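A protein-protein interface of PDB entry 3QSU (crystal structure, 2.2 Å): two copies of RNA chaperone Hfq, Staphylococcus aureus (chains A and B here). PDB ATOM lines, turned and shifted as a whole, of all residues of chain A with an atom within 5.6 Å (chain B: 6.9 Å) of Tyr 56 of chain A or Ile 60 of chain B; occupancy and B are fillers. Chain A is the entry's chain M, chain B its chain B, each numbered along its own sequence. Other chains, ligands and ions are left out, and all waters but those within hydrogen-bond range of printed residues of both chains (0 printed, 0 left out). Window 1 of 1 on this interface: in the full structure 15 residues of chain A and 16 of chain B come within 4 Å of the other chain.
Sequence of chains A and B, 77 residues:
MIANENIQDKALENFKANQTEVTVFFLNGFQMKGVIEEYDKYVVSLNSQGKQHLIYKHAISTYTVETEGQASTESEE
Hydrophobic or aromatic side chains of chain B within 4 Å of the printed part of chain A: Leu 27, Ile 60 and Tyr 63.
Hydrophobic or aromatic side chains of chain A within 4 Å of the printed part of chain B: Tyr 42, Val 43, Leu 54, Ile 55, Tyr 56, His 58 and Ala 59.
Among the printed residues, 16 pairs touch across the chains.
Among the printed residues, no Asp or Glu carboxylate lies within 4 Å of a Lys or Arg side-chain nitrogen of the other chain.
Among the printed residues, merely in contact across the chains: Leu 54 of chain A with Thr 62 of chain B (3.2 Å), Tyr 56 of chain A with Lys 57 of chain B (3.2 Å), Ile 55 of chain A with Ser 61 of chain B (3.4 Å), Ala 59 of chain A with Ser 61 of chain B (3.5 Å), Tyr 56 of chain A with Ile 60 of chain B (3.5 Å), Ala 59 of chain A with Leu 27 of chain B (3.6 Å), His 58 of chain A with His 58 of chain B (3.7 Å), Ile 55 of chain A with Thr 62 of chain B (3.8 Å), Val 43 of chain A with Gln 8 of chain B (3.8 Å) and Tyr 42 of chain A with Gln 8 of chain B (3.98 Å).
Tyr 56 of chain A touches five residues of chain B.
Of chain A, only Tyr 56 and His 58 come within 4 Å of Ile 60 of chain B.
Printed residues of chain A within 4 Å of Leu 27 of chain B: Ala 59.
Printed residues of chain A within 4 Å of His 58 of chain B: His 58.
Of the printed residues of chain B, Ala 59 of chain A touches Leu 27 (3.6 Å) and Ser 61 (3.5 Å).
The nearest residue of chain B that does not touch Tyr 56 of chain A is Leu 12 of chain B (4.6 Å).
The nearest residue of chain A that does not touch Ile 60 of chain B is Ala 59 of chain A (4.1 Å).
The nearest printed residue of chain B that does not touch Ile 55 of chain A is Tyr 63 of chain B (4.9 Å).
The backbone carbonyl oxygen (O) of Lys 57 of chain B lies close to a ring nitrogen (NE2) of His 58 of chain A, 3.2 Å away.
OE1 of Gln 8 of chain B lies within hydrogen-bond range of OH of Tyr 56 of chain A, 2.6 Å away.
The backbone carbonyl oxygen of Leu 54 of chain A is in hydrogen-bond range of the backbone NH of Tyr 63 of chain B (2.8 Å).
N of Tyr 56 of chain A lies within hydrogen-bond range of O of Ser 61 of chain B (2.8 Å).
OH of Tyr 56 of chain A is in hydrogen-bond range of OH of Tyr 63 of chain B (2.8 Å).
O of Ile 60 of chain B lies within hydrogen-bond range of NE2 of His 58 of chain A (2.7 Å).
The backbone carbonyl oxygen (O) of Asp 40 of chain B sits at hydrogen-bond distance from the side-chain amino group (NZ) of Lys 57 of chain B, at 2.9 Å.
O of Thr 62 of chain B sits at hydrogen-bond distance from N of Phe 25 of chain B (2.8 Å).
O of Tyr 42 of chain A sits at hydrogen-bond distance from N of Lys 57 of chain A (3.0 Å).
O of Val 44 of chain A sits at hydrogen-bond distance from N of Ile 55 of chain A.
OE1 of Gln 8 of chain B sits at hydrogen-bond distance from NZ of Lys 57 of chain B, 2.8 Å away.
The backbone carbonyl oxygen of Ala 59 of chain B lies within hydrogen-bond range of the backbone NH of Leu 27 of chain B (3.0 Å).
Tyr 56 of chain A touches Lys 57 of chain B, but with the chains exchanged Lys 57 of chain A does not touch Tyr 56 of chain B (11.6 Å).
His 58 of chain A touches Lys 57 of chain B, but with the chains exchanged Lys 57 of chain A does not touch His 58 of chain B (9.0 Å).
His 58 of chain A touches its own counterpart, His 58 of chain B.
His 58 of chain A touches Ile 60 of chain B, but with the chains exchanged Ile 60 of chain A does not touch His 58 of chain B (9.3 Å).
Positions printed for both chains: 43, 44, 55, 56, 57, 58, 59 and 60.
Of the 16 pairs that touch across the chains among the printed residues, 1 has its exchanged pair printed and touching as well.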
ATOM      1  N   TYR A  42     -21.400 -17.435   3.278  1.00  0.00           N
ATOM      2  CA  TYR A  42     -21.997 -18.749   3.549  1.00  0.00           C
ATOM      3  C   TYR A  42     -21.025 -19.928   3.648  1.00  0.00           C
ATOM      4  O   TYR A  42     -21.340 -20.951   4.256  1.00  0.00           O
ATOM      5  CB  TYR A  42     -23.103 -19.069   2.531  1.00  0.00           C
ATOM      6  CG  TYR A  42     -24.249 -18.078   2.571  1.00  0.00           C
ATOM      7  CD1 TYR A  42     -25.141 -18.061   3.628  1.00  0.00           C
ATOM      8  CD2 TYR A  42     -24.420 -17.146   1.554  1.00  0.00           C
ATOM      9  CE1 TYR A  42     -26.184 -17.144   3.669  1.00  0.00           C
ATOM     10  CE2 TYR A  42     -25.449 -16.227   1.582  1.00  0.00           C
ATOM     11  CZ  TYR A  42     -26.328 -16.231   2.635  1.00  0.00           C
ATOM     12  OH  TYR A  42     -27.353 -15.316   2.654  1.00  0.00           O
ATOM     13  N   VAL A  43     -19.845 -19.802   3.058  1.00  0.00           N
ATOM     14  CA  VAL A  43     -18.943 -20.938   3.017  1.00  0.00           C
ATOM     15  C   VAL A  43     -17.538 -20.550   3.387  1.00  0.00           C
ATOM     16  O   VAL A  43     -17.195 -19.370   3.435  1.00  0.00           O
ATOM     17  CB  VAL A  43     -18.901 -21.600   1.634  1.00  0.00           C
ATOM     18  CG1 VAL A  43     -20.269 -22.138   1.258  1.00  0.00           C
ATOM     19  CG2 VAL A  43     -18.410 -20.609   0.587  1.00  0.00           C
ATOM     20  N   VAL A  44     -16.735 -21.573   3.644  1.00  0.00           N
ATOM     21  CA  VAL A  44     -15.315 -21.422   3.881  1.00  0.00           C
ATOM     22  C   VAL A  44     -14.631 -22.492   3.063  1.00  0.00           C
ATOM     23  O   VAL A  44     -15.118 -23.620   2.985  1.00  0.00           O
ATOM     24  CB  VAL A  44     -14.974 -21.632   5.382  1.00  0.00           C
ATOM     25  CG1 VAL A  44     -13.482 -21.712   5.561  1.00  0.00           C
ATOM     26  CG2 VAL A  44     -15.511 -20.492   6.188  1.00  0.00           C
ATOM     27  N   LEU A  54     -14.991 -27.550   0.618  1.00  0.00           N
ATOM     28  CA  LEU A  54     -15.865 -26.395   0.641  1.00  0.00           C
ATOM     29  C   LEU A  54     -16.938 -26.672   1.673  1.00  0.00           C
ATOM     30  O   LEU A  54     -17.812 -27.517   1.461  1.00  0.00           O
ATOM     31  CB  LEU A  54     -16.507 -26.171  -0.726  1.00  0.00           C
ATOM     32  CG  LEU A  54     -17.204 -24.818  -0.872  1.00  0.00           C
ATOM     33  CD1 LEU A  54     -16.163 -23.703  -0.860  1.00  0.00           C
ATOM     34  CD2 LEU A  54     -18.055 -24.754  -2.149  1.00  0.00           C
ATOM     35  N   ILE A  55     -16.871 -25.944   2.783  1.00  0.00           N
ATOM     36  CA  ILE A  55     -17.686 -26.231   3.963  1.00  0.00           C
ATOM     37  C   ILE A  55     -18.722 -25.157   4.181  1.00  0.00           C
ATOM     38  O   ILE A  55     -18.373 -23.979   4.205  1.00  0.00           O
ATOM     39  CB  ILE A  55     -16.791 -26.232   5.241  1.00  0.00           C
ATOM     40  CG1 ILE A  55     -15.636 -27.230   5.092  1.00  0.00           C
ATOM     41  CG2 ILE A  55     -17.639 -26.499   6.486  1.00  0.00           C
ATOM     42  CD1 ILE A  55     -14.441 -26.943   5.969  1.00  0.00           C
ATOM     43  N   TYR A  56     -19.984 -25.547   4.362  1.00  0.00           N
ATOM     44  CA  TYR A  56     -21.017 -24.599   4.768  1.00  0.00           C
ATOM     45  C   TYR A  56     -20.866 -24.189   6.220  1.00  0.00           C
ATOM     46  O   TYR A  56     -20.693 -25.037   7.099  1.00  0.00           O
ATOM     47  CB  TYR A  56     -22.434 -25.172   4.567  1.00  0.00           C
ATOM     48  CG  TYR A  56     -22.873 -25.135   3.130  1.00  0.00           C
ATOM     49  CD1 TYR A  56     -23.146 -23.923   2.501  1.00  0.00           C
ATOM     50  CD2 TYR A  56     -22.987 -26.300   2.393  1.00  0.00           C
ATOM     51  CE1 TYR A  56     -23.532 -23.876   1.163  1.00  0.00           C
ATOM     52  CE2 TYR A  56     -23.377 -26.266   1.058  1.00  0.00           C
ATOM     53  CZ  TYR A  56     -23.643 -25.053   0.450  1.00  0.00           C
ATOM     54  OH  TYR A  56     -24.025 -25.019  -0.871  1.00  0.00           O
ATOM     55  N   LYS A  57     -20.984 -22.888   6.468  1.00  0.00           N
ATOM     56  CA  LYS A  57     -20.922 -22.367   7.821  1.00  0.00           C
ATOM     57  C   LYS A  57     -22.026 -22.949   8.699  1.00  0.00           C
ATOM     58  O   LYS A  57     -21.805 -23.201   9.884  1.00  0.00           O
ATOM     59  CB  LYS A  57     -20.984 -20.837   7.815  1.00  0.00           C
ATOM     60  CG  LYS A  57     -19.713 -20.164   7.290  1.00  0.00           C
ATOM     61  CD  LYS A  57     -19.842 -18.650   7.349  1.00  0.00           C
ATOM     62  CE  LYS A  57     -18.674 -17.972   6.647  1.00  0.00           C
ATOM     63  NZ  LYS A  57     -18.685 -16.491   6.811  1.00  0.00           N
ATOM     64  N   HIS A  58     -23.210 -23.175   8.128  1.00  0.00           N
ATOM     65  CA  HIS A  58     -24.336 -23.665   8.928  1.00  0.00           C
ATOM     66  C   HIS A  58     -23.971 -25.009   9.525  1.00  0.00           C
ATOM     67  O   HIS A  58     -24.569 -25.444  10.488  1.00  0.00           O
ATOM     68  CB  HIS A  58     -25.651 -23.752   8.107  1.00  0.00           C
ATOM     69  CG  HIS A  58     -25.629 -24.774   7.010  1.00  0.00           C
ATOM     70  ND1 HIS A  58     -25.996 -24.481   5.712  1.00  0.00           N
ATOM     71  CD2 HIS A  58     -25.309 -26.092   7.018  1.00  0.00           C
ATOM     72  CE1 HIS A  58     -25.882 -25.565   4.966  1.00  0.00           C
ATOM     73  NE2 HIS A  58     -25.474 -26.559   5.733  1.00  0.00           N
ATOM     74  N   ALA A  59     -22.973 -25.664   8.948  1.00  0.00           N
ATOM     75  CA  ALA A  59     -22.543 -26.969   9.438  1.00  0.00           C
ATOM     76  C   ALA A  59     -21.386 -26.888  10.438  1.00  0.00           C
ATOM     77  O   ALA A  59     -20.933 -27.910  10.947  1.00  0.00           O
ATOM     78  CB  ALA A  59     -22.140 -27.856   8.280  1.00  0.00           C
ATOM     79  N   ILE A  60     -20.901 -25.681  10.701  1.00  0.00           N
ATOM     80  CA  ILE A  60     -19.739 -25.524  11.576  1.00  0.00           C
ATOM     81  C   ILE A  60     -20.126 -25.151  13.010  1.00  0.00           C
ATOM     82  O   ILE A  60     -20.907 -24.226  13.249  1.00  0.00           O
ATOM     83  CB  ILE A  60     -18.775 -24.463  11.070  1.00  0.00           C
ATOM     84  CG1 ILE A  60     -18.160 -24.885   9.726  1.00  0.00           C
ATOM     85  CG2 ILE A  60     -17.667 -24.211  12.124  1.00  0.00           C
ATOM     86  CD1 ILE A  60     -17.107 -23.893   9.199  1.00  0.00           C
ATOM     87  N   GLN B   8     -18.949 -19.580  -3.075  1.00  0.00           N
ATOM     88  CA  GLN B   8     -19.881 -20.694  -3.233  1.00  0.00           C
ATOM     89  C   GLN B   8     -20.293 -20.894  -4.690  1.00  0.00           C
ATOM     90  O   GLN B   8     -20.259 -22.010  -5.205  1.00  0.00           O
ATOM     91  CB  GLN B   8     -21.144 -20.530  -2.370  1.00  0.00           C
ATOM     92  CG  GLN B   8     -22.024 -21.748  -2.513  1.00  0.00           C
ATOM     93  CD  GLN B   8     -23.372 -21.668  -1.814  1.00  0.00           C
ATOM     94  OE1 GLN B   8     -24.157 -22.605  -1.909  1.00  0.00           O
ATOM     95  NE2 GLN B   8     -23.646 -20.572  -1.114  1.00  0.00           N
ATOM     96  N   LEU B  12     -19.381 -23.978  -7.263  1.00  0.00           N
ATOM     97  CA  LEU B  12     -20.394 -24.850  -7.838  1.00  0.00           C
ATOM     98  C   LEU B  12     -20.365 -24.706  -9.358  1.00  0.00           C
ATOM     99  O   LEU B  12     -20.421 -25.690 -10.082  1.00  0.00           O
ATOM    100  CB  LEU B  12     -21.792 -24.513  -7.293  1.00  0.00           C
ATOM    101  CG  LEU B  12     -22.056 -24.669  -5.786  1.00  0.00           C
ATOM    102  CD1 LEU B  12     -23.518 -24.362  -5.442  1.00  0.00           C
ATOM    103  CD2 LEU B  12     -21.686 -26.063  -5.314  1.00  0.00           C
ATOM    104  N   VAL B  24     -19.932 -35.299  -1.548  1.00  0.00           N
ATOM    105  CA  VAL B  24     -20.778 -34.447  -0.719  1.00  0.00           C
ATOM    106  C   VAL B  24     -20.965 -35.089   0.648  1.00  0.00           C
ATOM    107  O   VAL B  24     -21.428 -36.227   0.743  1.00  0.00           O
ATOM    108  CB  VAL B  24     -22.178 -34.233  -1.347  1.00  0.00           C
ATOM    109  CG1 VAL B  24     -23.052 -33.420  -0.412  1.00  0.00           C
ATOM    110  CG2 VAL B  24     -22.086 -33.557  -2.710  1.00  0.00           C
ATOM    111  N   PHE B  25     -20.599 -34.371   1.705  1.00  0.00           N
ATOM    112  CA  PHE B  25     -20.846 -34.850   3.062  1.00  0.00           C
ATOM    113  C   PHE B  25     -22.072 -34.184   3.651  1.00  0.00           C
ATOM    114  O   PHE B  25     -22.229 -32.964   3.567  1.00  0.00           O
ATOM    115  CB  PHE B  25     -19.639 -34.597   3.973  1.00  0.00           C
ATOM    116  CG  PHE B  25     -18.458 -35.465   3.654  1.00  0.00           C
ATOM    117  CD1 PHE B  25     -18.334 -36.724   4.224  1.00  0.00           C
ATOM    118  CD2 PHE B  25     -17.476 -35.029   2.783  1.00  0.00           C
ATOM    119  CE1 PHE B  25     -17.249 -37.532   3.926  1.00  0.00           C
ATOM    120  CE2 PHE B  25     -16.381 -35.828   2.485  1.00  0.00           C
ATOM    121  CZ  PHE B  25     -16.269 -37.080   3.053  1.00  0.00           C
ATOM    122  N   PHE B  26     -22.928 -34.993   4.263  1.00  0.00           N
ATOM    123  CA  PHE B  26     -24.173 -34.514   4.854  1.00  0.00           C
ATOM    124  C   PHE B  26     -24.033 -34.274   6.354  1.00  0.00           C
ATOM    125  O   PHE B  26     -23.175 -34.864   7.009  1.00  0.00           O
ATOM    126  CB  PHE B  26     -25.301 -35.518   4.588  1.00  0.00           C
ATOM    127  CG  PHE B  26     -25.666 -35.632   3.133  1.00  0.00           C
ATOM    128  CD1 PHE B  26     -26.878 -35.143   2.668  1.00  0.00           C
ATOM    129  CD2 PHE B  26     -24.780 -36.198   2.225  1.00  0.00           C
ATOM    130  CE1 PHE B  26     -27.203 -35.232   1.329  1.00  0.00           C
ATOM    131  CE2 PHE B  26     -25.101 -36.291   0.883  1.00  0.00           C
ATOM    132  CZ  PHE B  26     -26.316 -35.808   0.433  1.00  0.00           C
ATOM    133  N   LEU B  27     -24.887 -33.407   6.884  1.00  0.00           N
ATOM    134  CA  LEU B  27     -24.896 -33.101   8.309  1.00  0.00           C
ATOM    135  C   LEU B  27     -24.856 -34.352   9.172  1.00  0.00           C
ATOM    136  O   LEU B  27     -24.116 -34.408  10.157  1.00  0.00           O
ATOM    137  CB  LEU B  27     -26.136 -32.278   8.674  1.00  0.00           C
ATOM    138  CG  LEU B  27     -26.176 -30.882   8.051  1.00  0.00           C
ATOM    139  CD1 LEU B  27     -27.326 -30.086   8.644  1.00  0.00           C
ATOM    140  CD2 LEU B  27     -24.845 -30.165   8.288  1.00  0.00           C
ATOM    141  N   ASP B  40     -29.352 -24.063  -7.526  1.00  0.00           N
ATOM    142  CA  ASP B  40     -29.806 -22.699  -7.300  1.00  0.00           C
ATOM    143  C   ASP B  40     -29.550 -22.339  -5.840  1.00  0.00           C
ATOM    144  O   ASP B  40     -28.713 -22.958  -5.187  1.00  0.00           O
ATOM    145  CB  ASP B  40     -31.281 -22.521  -7.672  1.00  0.00           C
ATOM    146  CG  ASP B  40     -32.193 -23.429  -6.890  1.00  0.00           C
ATOM    147  OD1 ASP B  40     -31.838 -23.790  -5.744  1.00  0.00           O
ATOM    148  OD2 ASP B  40     -33.275 -23.778  -7.418  1.00  0.00           O
ATOM    149  N   LYS B  41     -30.283 -21.362  -5.326  1.00  0.00           N
ATOM    150  CA  LYS B  41     -30.002 -20.828  -4.012  1.00  0.00           C
ATOM    151  C   LYS B  41     -30.187 -21.859  -2.904  1.00  0.00           C
ATOM    152  O   LYS B  41     -29.414 -21.884  -1.951  1.00  0.00           O
ATOM    153  CB  LYS B  41     -30.843 -19.573  -3.746  1.00  0.00           C
ATOM    154  CG  LYS B  41     -30.447 -18.388  -4.626  1.00  0.00           C
ATOM    155  CD  LYS B  41     -30.622 -17.059  -3.891  1.00  0.00           C
ATOM    156  CE  LYS B  41     -29.380 -16.175  -4.043  1.00  0.00           C
ATOM    157  NZ  LYS B  41     -29.082 -15.845  -5.478  1.00  0.00           N
ATOM    158  N   VAL B  43     -30.994 -25.492  -3.481  1.00  0.00           N
ATOM    159  CA  VAL B  43     -30.757 -26.902  -3.761  1.00  0.00           C
ATOM    160  C   VAL B  43     -29.606 -27.174  -4.713  1.00  0.00           C
ATOM    161  O   VAL B  43     -29.160 -26.309  -5.455  1.00  0.00           O
ATOM    162  CB  VAL B  43     -32.027 -27.609  -4.315  1.00  0.00           C
ATOM    163  CG1 VAL B  43     -33.218 -27.362  -3.399  1.00  0.00           C
ATOM    164  CG2 VAL B  43     -32.326 -27.134  -5.715  1.00  0.00           C
ATOM    165  N   VAL B  44     -29.140 -28.408  -4.675  1.00  0.00           N
ATOM    166  CA  VAL B  44     -28.127 -28.861  -5.587  1.00  0.00           C
ATOM    167  C   VAL B  44     -28.577 -30.171  -6.182  1.00  0.00           C
ATOM    168  O   VAL B  44     -29.071 -31.044  -5.477  1.00  0.00           O
ATOM    169  CB  VAL B  44     -26.779 -29.039  -4.877  1.00  0.00           C
ATOM    170  CG1 VAL B  44     -25.884 -29.934  -5.693  1.00  0.00           C
ATOM    171  CG2 VAL B  44     -26.152 -27.675  -4.654  1.00  0.00           C
ATOM    172  N   ILE B  55     -30.796 -32.242  -3.633  1.00  0.00           N
ATOM    173  CA  ILE B  55     -30.281 -32.089  -2.277  1.00  0.00           C
ATOM    174  C   ILE B  55     -30.483 -30.671  -1.774  1.00  0.00           C
ATOM    175  O   ILE B  55     -30.148 -29.731  -2.479  1.00  0.00           O
ATOM    176  CB  ILE B  55     -28.776 -32.430  -2.244  1.00  0.00           C
ATOM    177  CG1 ILE B  55     -28.544 -33.803  -2.879  1.00  0.00           C
ATOM    178  CG2 ILE B  55     -28.261 -32.422  -0.828  1.00  0.00           C
ATOM    179  CD1 ILE B  55     -27.107 -34.112  -3.180  1.00  0.00           C
ATOM    180  N   TYR B  56     -31.037 -30.517  -0.568  1.00  0.00           N
ATOM    181  CA  TYR B  56     -31.097 -29.207   0.095  1.00  0.00           C
ATOM    182  C   TYR B  56     -29.752 -28.756   0.655  1.00  0.00           C
ATOM    183  O   TYR B  56     -29.093 -29.502   1.368  1.00  0.00           O
ATOM    184  CB  TYR B  56     -32.114 -29.204   1.247  1.00  0.00           C
ATOM    185  CG  TYR B  56     -33.542 -29.143   0.779  1.00  0.00           C
ATOM    186  CD1 TYR B  56     -34.022 -28.025   0.106  1.00  0.00           C
ATOM    187  CD2 TYR B  56     -34.409 -30.206   0.990  1.00  0.00           C
ATOM    188  CE1 TYR B  56     -35.333 -27.969  -0.343  1.00  0.00           C
ATOM    189  CE2 TYR B  56     -35.729 -30.157   0.532  1.00  0.00           C
ATOM    190  CZ  TYR B  56     -36.176 -29.038  -0.130  1.00  0.00           C
ATOM    191  OH  TYR B  56     -37.473 -28.982  -0.577  1.00  0.00           O
ATOM    192  N   LYS B  57     -29.350 -27.527   0.357  1.00  0.00           N
ATOM    193  CA  LYS B  57     -28.107 -27.023   0.928  1.00  0.00           C
ATOM    194  C   LYS B  57     -28.087 -27.132   2.462  1.00  0.00           C
ATOM    195  O   LYS B  57     -27.027 -27.375   3.039  1.00  0.00           O
ATOM    196  CB  LYS B  57     -27.812 -25.598   0.463  1.00  0.00           C
ATOM    197  CG  LYS B  57     -27.372 -25.518  -1.009  1.00  0.00           C
ATOM    198  CD  LYS B  57     -27.086 -24.081  -1.417  1.00  0.00           C
ATOM    199  CE  LYS B  57     -26.600 -23.970  -2.839  1.00  0.00           C
ATOM    200  NZ  LYS B  57     -26.635 -22.551  -3.262  1.00  0.00           N
ATOM    201  N   HIS B  58     -29.248 -27.004   3.115  1.00  0.00           N
ATOM    202  CA  HIS B  58     -29.272 -27.087   4.565  1.00  0.00           C
ATOM    203  C   HIS B  58     -28.887 -28.479   5.047  1.00  0.00           C
ATOM    204  O   HIS B  58     -28.538 -28.659   6.204  1.00  0.00           O
ATOM    205  CB  HIS B  58     -30.623 -26.633   5.168  1.00  0.00           C
ATOM    206  CG  HIS B  58     -31.792 -27.495   4.793  1.00  0.00           C
ATOM    207  ND1 HIS B  58     -32.897 -26.999   4.134  1.00  0.00           N
ATOM    208  CD2 HIS B  58     -32.035 -28.813   4.992  1.00  0.00           C
ATOM    209  CE1 HIS B  58     -33.772 -27.971   3.947  1.00  0.00           C
ATOM    210  NE2 HIS B  58     -33.274 -29.083   4.454  1.00  0.00           N
ATOM    211  N   ALA B  59     -28.958 -29.468   4.170  1.00  0.00           N
ATOM    212  CA  ALA B  59     -28.554 -30.810   4.567  1.00  0.00           C
ATOM    213  C   ALA B  59     -27.043 -31.065   4.377  1.00  0.00           C
ATOM    214  O   ALA B  59     -26.530 -32.085   4.819  1.00  0.00           O
ATOM    215  CB  ALA B  59     -29.345 -31.825   3.783  1.00  0.00           C
ATOM    216  N   ILE B  60     -26.346 -30.156   3.701  1.00  0.00           N
ATOM    217  CA  ILE B  60     -24.955 -30.401   3.302  1.00  0.00           C
ATOM    218  C   ILE B  60     -23.937 -29.810   4.292  1.00  0.00           C
ATOM    219  O   ILE B  60     -24.103 -28.685   4.748  1.00  0.00           O
ATOM    220  CB  ILE B  60     -24.703 -29.875   1.848  1.00  0.00           C
ATOM    221  CG1 ILE B  60     -25.550 -30.670   0.833  1.00  0.00           C
ATOM    222  CG2 ILE B  60     -23.228 -29.922   1.474  1.00  0.00           C
ATOM    223  CD1 ILE B  60     -25.541 -30.090  -0.600  1.00  0.00           C
ATOM    224  N   SER B  61     -22.910 -30.587   4.641  1.00  0.00           N
ATOM    225  CA  SER B  61     -21.741 -30.067   5.382  1.00  0.00           C
ATOM    226  C   SER B  61     -20.636 -29.540   4.472  1.00  0.00           C
ATOM    227  O   SER B  61     -20.240 -28.374   4.539  1.00  0.00           O
ATOM    228  CB  SER B  61     -21.105 -31.169   6.228  1.00  0.00           C
ATOM    229  OG  SER B  61     -21.704 -31.236   7.503  1.00  0.00           O
ATOM    230  N   THR B  62     -20.134 -30.431   3.626  1.00  0.00           N
ATOM    231  CA  THR B  62     -18.924 -30.172   2.868  1.00  0.00           C
ATOM    232  C   THR B  62     -18.999 -30.748   1.464  1.00  0.00           C
ATOM    233  O   THR B  62     -19.580 -31.810   1.236  1.00  0.00           O
ATOM    234  CB  THR B  62     -17.680 -30.813   3.552  1.00  0.00           C
ATOM    235  OG1 THR B  62     -17.673 -30.511   4.951  1.00  0.00           O
ATOM    236  CG2 THR B  62     -16.394 -30.294   2.931  1.00  0.00           C
ATOM    237  N   TYR B  63     -18.393 -30.039   0.528  1.00  0.00           N
ATOM    238  CA  TYR B  63     -18.068 -30.627  -0.754  1.00  0.00           C
ATOM    239  C   TYR B  63     -16.563 -30.878  -0.774  1.00  0.00           C
ATOM    240  O   TYR B  63     -15.776 -29.981  -0.495  1.00  0.00           O
ATOM    241  CB  TYR B  63     -18.403 -29.679  -1.897  1.00  0.00           C
ATOM    242  CG  TYR B  63     -19.805 -29.124  -1.945  1.00  0.00           C
ATOM    243  CD1 TYR B  63     -20.811 -29.777  -2.646  1.00  0.00           C
ATOM    244  CD2 TYR B  63     -20.106 -27.907  -1.348  1.00  0.00           C
ATOM    245  CE1 TYR B  63     -22.093 -29.249  -2.723  1.00  0.00           C
ATOM    246  CE2 TYR B  63     -21.366 -27.369  -1.424  1.00  0.00           C
ATOM    247  CZ  TYR B  63     -22.362 -28.038  -2.116  1.00  0.00           C
ATOM    248  OH  TYR B  63     -23.622 -27.498  -2.170  1.00  0.00           O
